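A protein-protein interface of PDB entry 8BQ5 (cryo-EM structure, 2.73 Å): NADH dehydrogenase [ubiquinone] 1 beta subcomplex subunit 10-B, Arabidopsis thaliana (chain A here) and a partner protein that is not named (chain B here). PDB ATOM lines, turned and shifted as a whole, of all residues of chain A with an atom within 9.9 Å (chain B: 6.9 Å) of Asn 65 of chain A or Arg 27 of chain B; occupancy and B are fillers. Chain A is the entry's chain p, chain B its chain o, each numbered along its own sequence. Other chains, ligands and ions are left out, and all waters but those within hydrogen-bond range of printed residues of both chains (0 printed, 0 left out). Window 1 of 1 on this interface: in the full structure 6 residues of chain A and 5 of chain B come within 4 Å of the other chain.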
ATOM      1  N   TRP A  57      25.939 -27.673  31.231  1.00  0.00           N
ATOM      2  CA  TRP A  57      25.304 -28.289  30.072  1.00  0.00           C
ATOM      3  C   TRP A  57      23.997 -27.593  29.715  1.00  0.00           C
ATOM      4  O   TRP A  57      23.550 -27.660  28.565  1.00  0.00           O
ATOM      5  CB  TRP A  57      25.093 -29.778  30.328  1.00  0.00           C
ATOM      6  CG  TRP A  57      26.353 -30.568  30.155  1.00  0.00           C
ATOM      7  CD1 TRP A  57      27.067 -31.198  31.132  1.00  0.00           C
ATOM      8  CD2 TRP A  57      27.053 -30.805  28.928  1.00  0.00           C
ATOM      9  NE1 TRP A  57      28.167 -31.814  30.590  1.00  0.00           N
ATOM     10  CE2 TRP A  57      28.182 -31.590  29.239  1.00  0.00           C
ATOM     11  CE3 TRP A  57      26.835 -30.433  27.598  1.00  0.00           C
ATOM     12  CZ2 TRP A  57      29.088 -32.007  28.268  1.00  0.00           C
ATOM     13  CZ3 TRP A  57      27.736 -30.849  26.638  1.00  0.00           C
ATOM     14  CH2 TRP A  57      28.849 -31.628  26.977  1.00  0.00           C
ATOM     15  N   CYS A  58      23.370 -26.921  30.682  1.00  0.00           N
ATOM     16  CA  CYS A  58      22.246 -26.049  30.356  1.00  0.00           C
ATOM     17  C   CYS A  58      22.686 -24.927  29.425  1.00  0.00           C
ATOM     18  O   CYS A  58      22.053 -24.673  28.394  1.00  0.00           O
ATOM     19  CB  CYS A  58      21.630 -25.480  31.635  1.00  0.00           C
ATOM     20  SG  CYS A  58      20.072 -24.595  31.395  1.00  0.00           S
ATOM     21  N   TYR A  59      23.790 -24.258  29.764  1.00  0.00           N
ATOM     22  CA  TYR A  59      24.340 -23.212  28.910  1.00  0.00           C
ATOM     23  C   TYR A  59      24.681 -23.757  27.529  1.00  0.00           C
ATOM     24  O   TYR A  59      24.458 -23.097  26.508  1.00  0.00           O
ATOM     25  CB  TYR A  59      25.581 -22.605  29.574  1.00  0.00           C
ATOM     26  CG  TYR A  59      26.177 -21.421  28.845  1.00  0.00           C
ATOM     27  CD1 TYR A  59      25.741 -20.131  29.105  1.00  0.00           C
ATOM     28  CD2 TYR A  59      27.180 -21.595  27.901  1.00  0.00           C
ATOM     29  CE1 TYR A  59      26.284 -19.051  28.449  1.00  0.00           C
ATOM     30  CE2 TYR A  59      27.728 -20.520  27.236  1.00  0.00           C
ATOM     31  CZ  TYR A  59      27.275 -19.248  27.515  1.00  0.00           C
ATOM     32  OH  TYR A  59      27.810 -18.167  26.861  1.00  0.00           O
ATOM     33  N   ARG A  60      25.239 -24.967  27.490  1.00  0.00           N
ATOM     34  CA  ARG A  60      25.705 -25.544  26.199  1.00  0.00           C
ATOM     35  C   ARG A  60      24.520 -26.004  25.343  1.00  0.00           C
ATOM     36  O   ARG A  60      24.611 -25.871  24.113  1.00  0.00           O
ATOM     37  CB  ARG A  60      26.676 -26.692  26.475  1.00  0.00           C
ATOM     38  CG  ARG A  60      27.990 -26.231  27.090  1.00  0.00           C
ATOM     39  CD  ARG A  60      28.887 -27.370  27.519  1.00  0.00           C
ATOM     40  NE  ARG A  60      30.170 -26.870  27.988  1.00  0.00           N
ATOM     41  CZ  ARG A  60      31.202 -27.636  28.311  1.00  0.00           C
ATOM     42  NH1 ARG A  60      31.106 -28.950  28.209  1.00  0.00           N
ATOM     43  NH2 ARG A  60      32.327 -27.088  28.729  1.00  0.00           N
ATOM     44  N   VAL A  61      23.470 -26.542  25.965  1.00  0.00           N
ATOM     45  CA  VAL A  61      22.342 -27.058  25.197  1.00  0.00           C
ATOM     46  C   VAL A  61      21.452 -25.924  24.699  1.00  0.00           C
ATOM     47  O   VAL A  61      21.024 -25.921  23.540  1.00  0.00           O
ATOM     48  CB  VAL A  61      21.551 -28.075  26.041  1.00  0.00           C
ATOM     49  CG1 VAL A  61      20.120 -28.202  25.540  1.00  0.00           C
ATOM     50  CG2 VAL A  61      22.244 -29.425  26.026  1.00  0.00           C
ATOM     51  N   GLU A  62      21.169 -24.943  25.553  1.00  0.00           N
ATOM     52  CA  GLU A  62      20.149 -23.944  25.268  1.00  0.00           C
ATOM     53  C   GLU A  62      20.657 -22.751  24.468  1.00  0.00           C
ATOM     54  O   GLU A  62      19.836 -21.987  23.950  1.00  0.00           O
ATOM     55  CB  GLU A  62      19.526 -23.453  26.577  1.00  0.00           C
ATOM     56  CG  GLU A  62      18.988 -24.575  27.450  1.00  0.00           C
ATOM     57  CD  GLU A  62      17.693 -25.161  26.920  1.00  0.00           C
ATOM     58  OE1 GLU A  62      17.266 -26.216  27.433  1.00  0.00           O
ATOM     59  OE2 GLU A  62      17.098 -24.564  25.999  1.00  0.00           O
ATOM     60  N   GLY A  63      21.971 -22.574  24.348  1.00  0.00           N
ATOM     61  CA  GLY A  63      22.497 -21.478  23.549  1.00  0.00           C
ATOM     62  C   GLY A  63      22.042 -20.123  24.052  1.00  0.00           C
ATOM     63  O   GLY A  63      22.108 -19.817  25.247  1.00  0.00           O
ATOM     64  N   VAL A  64      21.615 -19.270  23.117  1.00  0.00           N
ATOM     65  CA  VAL A  64      21.164 -17.883  23.464  1.00  0.00           C
ATOM     66  C   VAL A  64      19.871 -17.895  24.288  1.00  0.00           C
ATOM     67  O   VAL A  64      19.460 -16.810  24.735  1.00  0.00           O
ATOM     68  CB  VAL A  64      20.976 -17.034  22.196  1.00  0.00           C
ATOM     69  CG1 VAL A  64      22.246 -16.955  21.367  1.00  0.00           C
ATOM     70  CG2 VAL A  64      19.812 -17.520  21.350  1.00  0.00           C
ATOM     71  N   ASN A  65      19.261 -19.062  24.502  1.00  0.00           N
ATOM     72  CA  ASN A  65      18.055 -19.131  25.367  1.00  0.00           C
ATOM     73  C   ASN A  65      18.426 -19.544  26.796  1.00  0.00           C
ATOM     74  O   ASN A  65      17.504 -19.903  27.535  1.00  0.00           O
ATOM     75  CB  ASN A  65      17.002 -20.059  24.751  1.00  0.00           C
ATOM     76  CG  ASN A  65      16.680 -19.694  23.320  1.00  0.00           C
ATOM     77  OD1 ASN A  65      16.363 -18.546  23.026  1.00  0.00           O
ATOM     78  ND2 ASN A  65      16.776 -20.661  22.425  1.00  0.00           N
ATOM     79  N   HIS A  66      19.698 -19.430  27.160  1.00  0.00           N
ATOM     80  CA  HIS A  66      20.158 -19.904  28.493  1.00  0.00           C
ATOM     81  C   HIS A  66      19.664 -18.987  29.614  1.00  0.00           C
ATOM     82  O   HIS A  66      19.346 -19.510  30.675  1.00  0.00           O
ATOM     83  CB  HIS A  66      21.680 -20.064  28.473  1.00  0.00           C
ATOM     84  CG  HIS A  66      22.448 -18.795  28.615  1.00  0.00           C
ATOM     85  ND1 HIS A  66      22.880 -18.334  29.840  1.00  0.00           N
ATOM     86  CD2 HIS A  66      22.871 -17.899  27.700  1.00  0.00           C
ATOM     87  CE1 HIS A  66      23.533 -17.206  29.672  1.00  0.00           C
ATOM     88  NE2 HIS A  66      23.543 -16.917  28.369  1.00  0.00           N
ATOM     89  N   TYR A  67      19.586 -17.674  29.389  1.00  0.00           N
ATOM     90  CA  TYR A  67      19.214 -16.744  30.490  1.00  0.00           C
ATOM     91  C   TYR A  67      17.806 -17.060  30.994  1.00  0.00           C
ATOM     92  O   TYR A  67      17.593 -17.029  32.214  1.00  0.00           O
ATOM     93  CB  TYR A  67      19.316 -15.290  30.035  1.00  0.00           C
ATOM     94  CG  TYR A  67      20.709 -14.725  30.033  1.00  0.00           C
ATOM     95  CD1 TYR A  67      21.480 -14.733  31.182  1.00  0.00           C
ATOM     96  CD2 TYR A  67      21.257 -14.190  28.881  1.00  0.00           C
ATOM     97  CE1 TYR A  67      22.767 -14.226  31.185  1.00  0.00           C
ATOM     98  CE2 TYR A  67      22.540 -13.672  28.867  1.00  0.00           C
ATOM     99  CZ  TYR A  67      23.299 -13.699  30.023  1.00  0.00           C
ATOM    100  OH  TYR A  67      24.566 -13.200  30.027  1.00  0.00           O
ATOM    101  N   GLN A  68      16.883 -17.358  30.077  1.00  0.00           N
ATOM    102  CA  GLN A  68      15.481 -17.661  30.449  1.00  0.00           C
ATOM    103  C   GLN A  68      15.352 -19.125  30.873  1.00  0.00           C
ATOM    104  O   GLN A  68      14.544 -19.387  31.777  1.00  0.00           O
ATOM    105  CB  GLN A  68      14.602 -17.310  29.245  1.00  0.00           C
ATOM    106  CG  GLN A  68      13.100 -17.412  29.458  1.00  0.00           C
ATOM    107  CD  GLN A  68      12.363 -16.878  28.256  1.00  0.00           C
ATOM    108  OE1 GLN A  68      12.961 -16.355  27.318  1.00  0.00           O
ATOM    109  NE2 GLN A  68      11.045 -16.989  28.289  1.00  0.00           N
ATOM    110  N   LYS A  69      16.162 -20.027  30.309  1.00  0.00           N
ATOM    111  CA  LYS A  69      15.984 -21.484  30.571  1.00  0.00           C
ATOM    112  C   LYS A  69      16.794 -21.977  31.775  1.00  0.00           C
ATOM    113  O   LYS A  69      16.277 -22.852  32.493  1.00  0.00           O
ATOM    114  CB  LYS A  69      16.350 -22.289  29.323  1.00  0.00           C
ATOM    115  CG  LYS A  69      15.164 -22.835  28.544  1.00  0.00           C
ATOM    116  CD  LYS A  69      14.641 -21.868  27.506  1.00  0.00           C
ATOM    117  CE  LYS A  69      13.702 -22.513  26.511  1.00  0.00           C
ATOM    118  NZ  LYS A  69      13.764 -21.850  25.186  1.00  0.00           N
ATOM    119  N   CYS A  70      18.006 -21.458  31.987  1.00  0.00           N
ATOM    120  CA  CYS A  70      18.879 -21.938  33.091  1.00  0.00           C
ATOM    121  C   CYS A  70      18.736 -21.056  34.328  1.00  0.00           C
ATOM    122  O   CYS A  70      19.474 -21.301  35.292  1.00  0.00           O
ATOM    123  CB  CYS A  70      20.339 -21.890  32.664  1.00  0.00           C
ATOM    124  SG  CYS A  70      20.627 -22.680  31.063  1.00  0.00           S
ATOM    125  N   ARG A  71      17.843 -20.063  34.295  1.00  0.00           N
ATOM    126  CA  ARG A  71      17.646 -19.118  35.429  1.00  0.00           C
ATOM    127  C   ARG A  71      17.621 -19.861  36.769  1.00  0.00           C
ATOM    128  O   ARG A  71      18.333 -19.422  37.694  1.00  0.00           O
ATOM    129  CB  ARG A  71      16.319 -18.384  35.232  1.00  0.00           C
ATOM    130  CG  ARG A  71      16.351 -16.908  35.597  1.00  0.00           C
ATOM    131  CD  ARG A  71      14.953 -16.397  35.886  1.00  0.00           C
ATOM    132  NE  ARG A  71      14.584 -16.610  37.279  1.00  0.00           N
ATOM    133  CZ  ARG A  71      14.675 -15.695  38.238  1.00  0.00           C
ATOM    134  NH1 ARG A  71      15.121 -14.480  37.964  1.00  0.00           N
ATOM    135  NH2 ARG A  71      14.318 -16.000  39.471  1.00  0.00           N
ATOM    136  N   HIS A  72      16.841 -20.939  36.866  1.00  0.00           N
ATOM    137  CA  HIS A  72      16.678 -21.703  38.132  1.00  0.00           C
ATOM    138  C   HIS A  72      17.983 -22.408  38.522  1.00  0.00           C
ATOM    139  O   HIS A  72      18.340 -22.331  39.704  1.00  0.00           O
ATOM    140  CB  HIS A  72      15.501 -22.686  37.994  1.00  0.00           C
ATOM    141  CG  HIS A  72      15.731 -23.796  37.022  1.00  0.00           C
ATOM    142  ND1 HIS A  72      15.783 -25.119  37.417  1.00  0.00           N
ATOM    143  CD2 HIS A  72      15.941 -23.792  35.687  1.00  0.00           C
ATOM    144  CE1 HIS A  72      16.001 -25.881  36.365  1.00  0.00           C
ATOM    145  NE2 HIS A  72      16.109 -25.091  35.293  1.00  0.00           N
ATOM    146  N   VAL A  74      21.068 -21.693  37.706  1.00  0.00           N
ATOM    147  CA  VAL A  74      22.067 -20.662  38.112  1.00  0.00           C
ATOM    148  C   VAL A  74      21.796 -20.293  39.572  1.00  0.00           C
ATOM    149  O   VAL A  74      22.733 -20.413  40.371  1.00  0.00           O
ATOM    150  CB  VAL A  74      22.036 -19.453  37.157  1.00  0.00           C
ATOM    151  CG1 VAL A  74      22.745 -18.232  37.711  1.00  0.00           C
ATOM    152  CG2 VAL A  74      22.579 -19.812  35.786  1.00  0.00           C
ATOM    153  N   MET B  10       4.257  -6.387  17.503  1.00  0.00           N
ATOM    154  CA  MET B  10       4.943  -7.668  17.601  1.00  0.00           C
ATOM    155  C   MET B  10       4.136  -8.760  16.910  1.00  0.00           C
ATOM    156  O   MET B  10       2.950  -8.950  17.198  1.00  0.00           O
ATOM    157  CB  MET B  10       5.184  -8.037  19.063  1.00  0.00           C
ATOM    158  CG  MET B  10       6.477  -8.806  19.306  1.00  0.00           C
ATOM    159  SD  MET B  10       7.828  -8.274  18.238  1.00  0.00           S
ATOM    160  CE  MET B  10       9.067  -9.514  18.604  1.00  0.00           C
ATOM    161  N   GLN B  14       7.287 -15.107  21.691  1.00  0.00           N
ATOM    162  CA  GLN B  14       8.508 -15.436  22.418  1.00  0.00           C
ATOM    163  C   GLN B  14       8.999 -16.834  22.072  1.00  0.00           C
ATOM    164  O   GLN B  14      10.206 -17.057  21.919  1.00  0.00           O
ATOM    165  CB  GLN B  14       8.270 -15.320  23.922  1.00  0.00           C
ATOM    166  CG  GLN B  14       8.281 -13.906  24.454  1.00  0.00           C
ATOM    167  CD  GLN B  14       7.469 -13.762  25.722  1.00  0.00           C
ATOM    168  OE1 GLN B  14       6.523 -14.513  25.955  1.00  0.00           O
ATOM    169  NE2 GLN B  14       7.844 -12.804  26.558  1.00  0.00           N
ATOM    170  N   GLU B  15       8.078 -17.794  21.958  1.00  0.00           N
ATOM    171  CA  GLU B  15       8.475 -19.160  21.638  1.00  0.00           C
ATOM    172  C   GLU B  15       9.101 -19.232  20.252  1.00  0.00           C
ATOM    173  O   GLU B  15      10.146 -19.863  20.062  1.00  0.00           O
ATOM    174  CB  GLU B  15       7.262 -20.088  21.743  1.00  0.00           C
ATOM    175  CG  GLU B  15       7.539 -21.594  21.689  1.00  0.00           C
ATOM    176  CD  GLU B  15       8.915 -21.996  22.216  1.00  0.00           C
ATOM    177  OE1 GLU B  15       9.915 -21.865  21.487  1.00  0.00           O
ATOM    178  OE2 GLU B  15       9.010 -22.405  23.389  1.00  0.00           O
ATOM    179  N   GLU B  16       8.499 -18.554  19.274  1.00  0.00           N
ATOM    180  CA  GLU B  16       9.025 -18.610  17.914  1.00  0.00           C
ATOM    181  C   GLU B  16      10.436 -18.038  17.842  1.00  0.00           C
ATOM    182  O   GLU B  16      11.306 -18.595  17.162  1.00  0.00           O
ATOM    183  CB  GLU B  16       8.088 -17.867  16.966  1.00  0.00           C
ATOM    184  CG  GLU B  16       6.685 -18.444  16.913  1.00  0.00           C
ATOM    185  CD  GLU B  16       6.594 -19.659  16.010  1.00  0.00           C
ATOM    186  OE1 GLU B  16       6.775 -20.789  16.510  1.00  0.00           O
ATOM    187  OE2 GLU B  16       6.351 -19.483  14.799  1.00  0.00           O
ATOM    188  N   MET B  17      10.665 -16.905  18.508  1.00  0.00           N
ATOM    189  CA  MET B  17      12.037 -16.323  18.544  1.00  0.00           C
ATOM    190  C   MET B  17      12.980 -17.254  19.316  1.00  0.00           C
ATOM    191  O   MET B  17      14.116 -17.449  18.854  1.00  0.00           O
ATOM    192  CB  MET B  17      12.027 -14.947  19.204  1.00  0.00           C
ATOM    193  CG  MET B  17      11.198 -13.932  18.463  1.00  0.00           C
ATOM    194  SD  MET B  17      11.266 -12.332  19.288  1.00  0.00           S
ATOM    195  CE  MET B  17      10.796 -12.795  20.953  1.00  0.00           C
ATOM    196  N   SER B  18      12.523 -17.826  20.432  1.00  0.00           N
ATOM    197  CA  SER B  18      13.346 -18.790  21.211  1.00  0.00           C
ATOM    198  C   SER B  18      13.640 -20.038  20.372  1.00  0.00           C
ATOM    199  O   SER B  18      14.753 -20.566  20.484  1.00  0.00           O
ATOM    200  CB  SER B  18      12.661 -19.160  22.486  1.00  0.00           C
ATOM    201  OG  SER B  18      12.465 -18.020  23.307  1.00  0.00           O
ATOM    202  N   ALA B  19      12.686 -20.476  19.547  1.00  0.00           N
ATOM    203  CA  ALA B  19      12.861 -21.697  18.725  1.00  0.00           C
ATOM    204  C   ALA B  19      13.852 -21.422  17.594  1.00  0.00           C
ATOM    205  O   ALA B  19      14.620 -22.335  17.261  1.00  0.00           O
ATOM    206  CB  ALA B  19      11.528 -22.163  18.199  1.00  0.00           C
ATOM    207  N   ALA B  20      13.853 -20.204  17.055  1.00  0.00           N
ATOM    208  CA  ALA B  20      14.804 -19.832  15.984  1.00  0.00           C
ATOM    209  C   ALA B  20      16.136 -19.387  16.595  1.00  0.00           C
ATOM    210  O   ALA B  20      16.944 -18.821  15.834  1.00  0.00           O
ATOM    211  CB  ALA B  20      14.207 -18.747  15.137  1.00  0.00           C
ATOM    212  N   LYS B  21      16.355 -19.645  17.890  1.00  0.00           N
ATOM    213  CA  LYS B  21      17.606 -19.258  18.598  1.00  0.00           C
ATOM    214  C   LYS B  21      18.036 -17.861  18.132  1.00  0.00           C
ATOM    215  O   LYS B  21      19.173 -17.722  17.637  1.00  0.00           O
ATOM    216  CB  LYS B  21      18.670 -20.334  18.366  1.00  0.00           C
ATOM    217  CG  LYS B  21      18.321 -21.716  18.902  1.00  0.00           C
ATOM    218  CD  LYS B  21      19.429 -22.730  18.715  1.00  0.00           C
ATOM    219  CE  LYS B  21      20.622 -22.488  19.614  1.00  0.00           C
ATOM    220  NZ  LYS B  21      20.292 -22.728  21.039  1.00  0.00           N
ATOM    221  N   ILE B  22      17.161 -16.865  18.297  1.00  0.00           N
ATOM    222  CA  ILE B  22      17.463 -15.485  17.814  1.00  0.00           C
ATOM    223  C   ILE B  22      18.329 -14.775  18.859  1.00  0.00           C
ATOM    224  O   ILE B  22      17.970 -14.828  20.048  1.00  0.00           O
ATOM    225  CB  ILE B  22      16.153 -14.725  17.526  1.00  0.00           C
ATOM    226  CG1 ILE B  22      15.349 -15.388  16.406  1.00  0.00           C
ATOM    227  CG2 ILE B  22      16.402 -13.258  17.222  1.00  0.00           C
ATOM    228  CD1 ILE B  22      15.952 -15.223  15.033  1.00  0.00           C
ATOM    229  N   ALA B  23      19.416 -14.132  18.428  1.00  0.00           N
ATOM    230  CA  ALA B  23      20.261 -13.344  19.354  1.00  0.00           C
ATOM    231  C   ALA B  23      19.386 -12.358  20.127  1.00  0.00           C
ATOM    232  O   ALA B  23      18.519 -11.732  19.506  1.00  0.00           O
ATOM    233  CB  ALA B  23      21.330 -12.637  18.570  1.00  0.00           C
ATOM    234  N   LEU B  24      19.639 -12.193  21.422  1.00  0.00           N
ATOM    235  CA  LEU B  24      18.804 -11.345  22.267  1.00  0.00           C
ATOM    236  C   LEU B  24      18.742  -9.913  21.751  1.00  0.00           C
ATOM    237  O   LEU B  24      17.773  -9.192  22.013  1.00  0.00           O
ATOM    238  CB  LEU B  24      19.325 -11.374  23.703  1.00  0.00           C
ATOM    239  CG  LEU B  24      19.192 -12.714  24.427  1.00  0.00           C
ATOM    240  CD1 LEU B  24      19.547 -12.560  25.892  1.00  0.00           C
ATOM    241  CD2 LEU B  24      17.787 -13.275  24.271  1.00  0.00           C
ATOM    242  N   GLY B  25      19.765  -9.481  21.018  1.00  0.00           N
ATOM    243  CA  GLY B  25      19.742  -8.143  20.457  1.00  0.00           C
ATOM    244  C   GLY B  25      18.873  -7.993  19.227  1.00  0.00           C
ATOM    245  O   GLY B  25      18.635  -6.860  18.796  1.00  0.00           O
ATOM    246  N   SER B  26      18.368  -9.099  18.681  1.00  0.00           N
ATOM    247  CA  SER B  26      17.605  -9.044  17.404  1.00  0.00           C
ATOM    248  C   SER B  26      16.136  -9.403  17.637  1.00  0.00           C
ATOM    249  O   SER B  26      15.443  -9.723  16.653  1.00  0.00           O
ATOM    250  CB  SER B  26      18.245  -9.958  16.402  1.00  0.00           C
ATOM    251  OG  SER B  26      19.579  -9.562  16.130  1.00  0.00           O
ATOM    252  N   ARG B  27      15.680  -9.392  18.892  1.00  0.00           N
ATOM    253  CA  ARG B  27      14.258  -9.668  19.207  1.00  0.00           C
ATOM    254  C   ARG B  27      13.512  -8.331  19.168  1.00  0.00           C
ATOM    255  O   ARG B  27      12.883  -7.980  20.173  1.00  0.00           O
ATOM    256  CB  ARG B  27      14.173 -10.394  20.553  1.00  0.00           C
ATOM    257  CG  ARG B  27      15.159 -11.546  20.702  1.00  0.00           C
ATOM    258  CD  ARG B  27      14.712 -12.670  21.616  1.00  0.00           C
ATOM    259  NE  ARG B  27      15.284 -13.938  21.188  1.00  0.00           N
ATOM    260  CZ  ARG B  27      15.190 -15.091  21.843  1.00  0.00           C
ATOM    261  NH1 ARG B  27      14.536 -15.163  22.988  1.00  0.00           N
ATOM    262  NH2 ARG B  27      15.757 -16.174  21.347  1.00  0.00           N
ATOM    263  N   ASP B  28      13.603  -7.606  18.050  1.00  0.00           N
ATOM    264  CA  ASP B  28      12.971  -6.266  17.899  1.00  0.00           C
ATOM    265  C   ASP B  28      11.529  -6.408  17.406  1.00  0.00           C
ATOM    266  O   ASP B  28      10.799  -7.197  17.990  1.00  0.00           O
ATOM    267  CB  ASP B  28      13.797  -5.384  16.957  1.00  0.00           C
ATOM    268  CG  ASP B  28      13.929  -5.938  15.548  1.00  0.00           C
ATOM    269  OD1 ASP B  28      13.441  -7.057  15.306  1.00  0.00           O
ATOM    270  OD2 ASP B  28      14.534  -5.248  14.710  1.00  0.00           O
ATOM    271  N   MET B  29      11.137  -5.636  16.393  1.00  0.00           N
ATOM    272  CA  MET B  29       9.772  -5.741  15.815  1.00  0.00           C
ATOM    273  C   MET B  29       9.856  -6.453  14.463  1.00  0.00           C
ATOM    274  O   MET B  29       8.798  -6.841  13.936  1.00  0.00           O
ATOM    275  CB  MET B  29       9.135  -4.360  15.625  1.00  0.00           C
ATOM    276  CG  MET B  29       8.716  -3.704  16.926  1.00  0.00           C
ATOM    277  SD  MET B  29       7.043  -4.186  17.428  1.00  0.00           S
ATOM    278  CE  MET B  29       7.077  -3.749  19.164  1.00  0.00           C
ATOM    279  N   CYS B  30      11.072  -6.651  13.951  1.00  0.00           N
ATOM    280  CA  CYS B  30      11.210  -7.398  12.676  1.00  0.00           C
ATOM    281  C   CYS B  30      11.750  -8.802  12.931  1.00  0.00           C
ATOM    282  O   CYS B  30      12.373  -9.383  12.027  1.00  0.00           O
ATOM    283  CB  CYS B  30      12.103  -6.676  11.685  1.00  0.00           C
ATOM    284  SG  CYS B  30      11.622  -7.140  10.003  1.00  0.00           S
ATOM    285  N   ALA B  31      11.503  -9.329  14.122  1.00  0.00           N
ATOM    286  CA  ALA B  31      11.915 -10.717  14.401  1.00  0.00           C
ATOM    287  C   ALA B  31      11.224 -11.667  13.421  1.00  0.00           C
ATOM    288  O   ALA B  31      11.838 -12.695  13.073  1.00  0.00           O
ATOM    289  CB  ALA B  31      11.557 -11.039  15.814  1.00  0.00           C
ATOM    290  N   LEU B  34      13.150 -11.995  10.208  1.00  0.00           N
ATOM    291  CA  LEU B  34      14.520 -12.533  10.427  1.00  0.00           C
ATOM    292  C   LEU B  34      14.506 -14.063  10.344  1.00  0.00           C
ATOM    293  O   LEU B  34      15.458 -14.614   9.779  1.00  0.00           O
ATOM    294  CB  LEU B  34      15.008 -12.074  11.803  1.00  0.00           C
ATOM    295  CG  LEU B  34      16.469 -12.396  12.123  1.00  0.00           C
ATOM    296  CD1 LEU B  34      17.387 -11.959  10.992  1.00  0.00           C
ATOM    297  CD2 LEU B  34      16.890 -11.749  13.432  1.00  0.00           C
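ND2 of Asn 65 of chain A is in hydrogen-bond range of O of Ser 18 of chain B. The backbone carbonyl oxygen (O) of Glu 62 of chain A sits at hydrogen-bond distance from the side-chain amino group (NZ) of Lys 21 of chain B (3.0 Å). The guanidinium group (NH2) of Arg 27 of chain B sits at hydrogen-bond distance from the side-chain amide oxygen (OD1) of Asn 65 of chain A (3.0 Å).
OG of Ser 18 of chain B is in hydrogen-bond range of O of Gln 14 of chain B (2.8 Å). N of Ile 22 of chain B lies within hydrogen-bond range of O of Met 17 of chain B (3.2 Å). NH2 of Arg 27 of chain B sits at hydrogen-bond distance from O of Met 17 of chain B, 3.2 Å away. O of Ile 22 of chain B sits at hydrogen-bond distance from NH2 of Arg 27 of chain B (2.9 Å). The side-chain sulfur (SG) of Cys 58 of chain A forms a disulfide with the side-chain sulfur (SG) of Cys 70 of chain A (2.0 Å).
Among the printed residues, merely in contact across the chains: Gly 63 of chain A with Lys 21 of chain B (3.6 Å), Val 64 of chain A with Lys 21 of chain B (3.7 Å), Val 64 of chain A with Ile 22 of chain B (3.5 Å), Val 64 of chain A with Leu 24 of chain B (3.9 Å), Asn 65 of chain A with Lys 21 of chain B (3.99 Å), Tyr 67 of chain A with Leu 24 of chain B (3.8 Å) and Lys 69 of chain A with Ser 18 of chain B (3.97 Å).
Trp 57 of chain A touches none of the printed residues of chain B. Of the printed residues of chain B, Gly 63 of chain A touches Lys 21. Of the printed residues of chain B, Val 64 of chain A touches Lys 21, Ile 22 and Leu 24. Of the printed residues of chain B, Asn 65 of chain A touches Ser 18 (2.8 Å), Lys 21 (3.99 Å) and Arg 27 (3.0 Å). Of the printed residues of chain B, Tyr 67 of chain A touches Leu 24. Printed residues of chain B within 4 Å of Lys 69 of chain A: Ser 18 (3.97 Å). Val 74 of chain A touches none of the printed residues of chain B. Printed residues of chain A within 4 Å of Ser 18 of chain B: Asn 65 and Lys 69. Printed residues of chain A within 4 Å of Ile 22 of chain B: Val 64. No residue of chain A comes within 4 Å of Gly 25 of chain B. No residue of chain A comes within 4 Å of Ser 26 of chain B. Arg 27 of chain B touches one residue of chain A. No residue of chain A comes within 4 Å of Asp 28 of chain B.
Of the 17 printed residues of chain A, 6 touch a printed residue of chain B. Hydrophobic or aromatic side chains of chain B that line the printed part of chain A: Leu 24.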
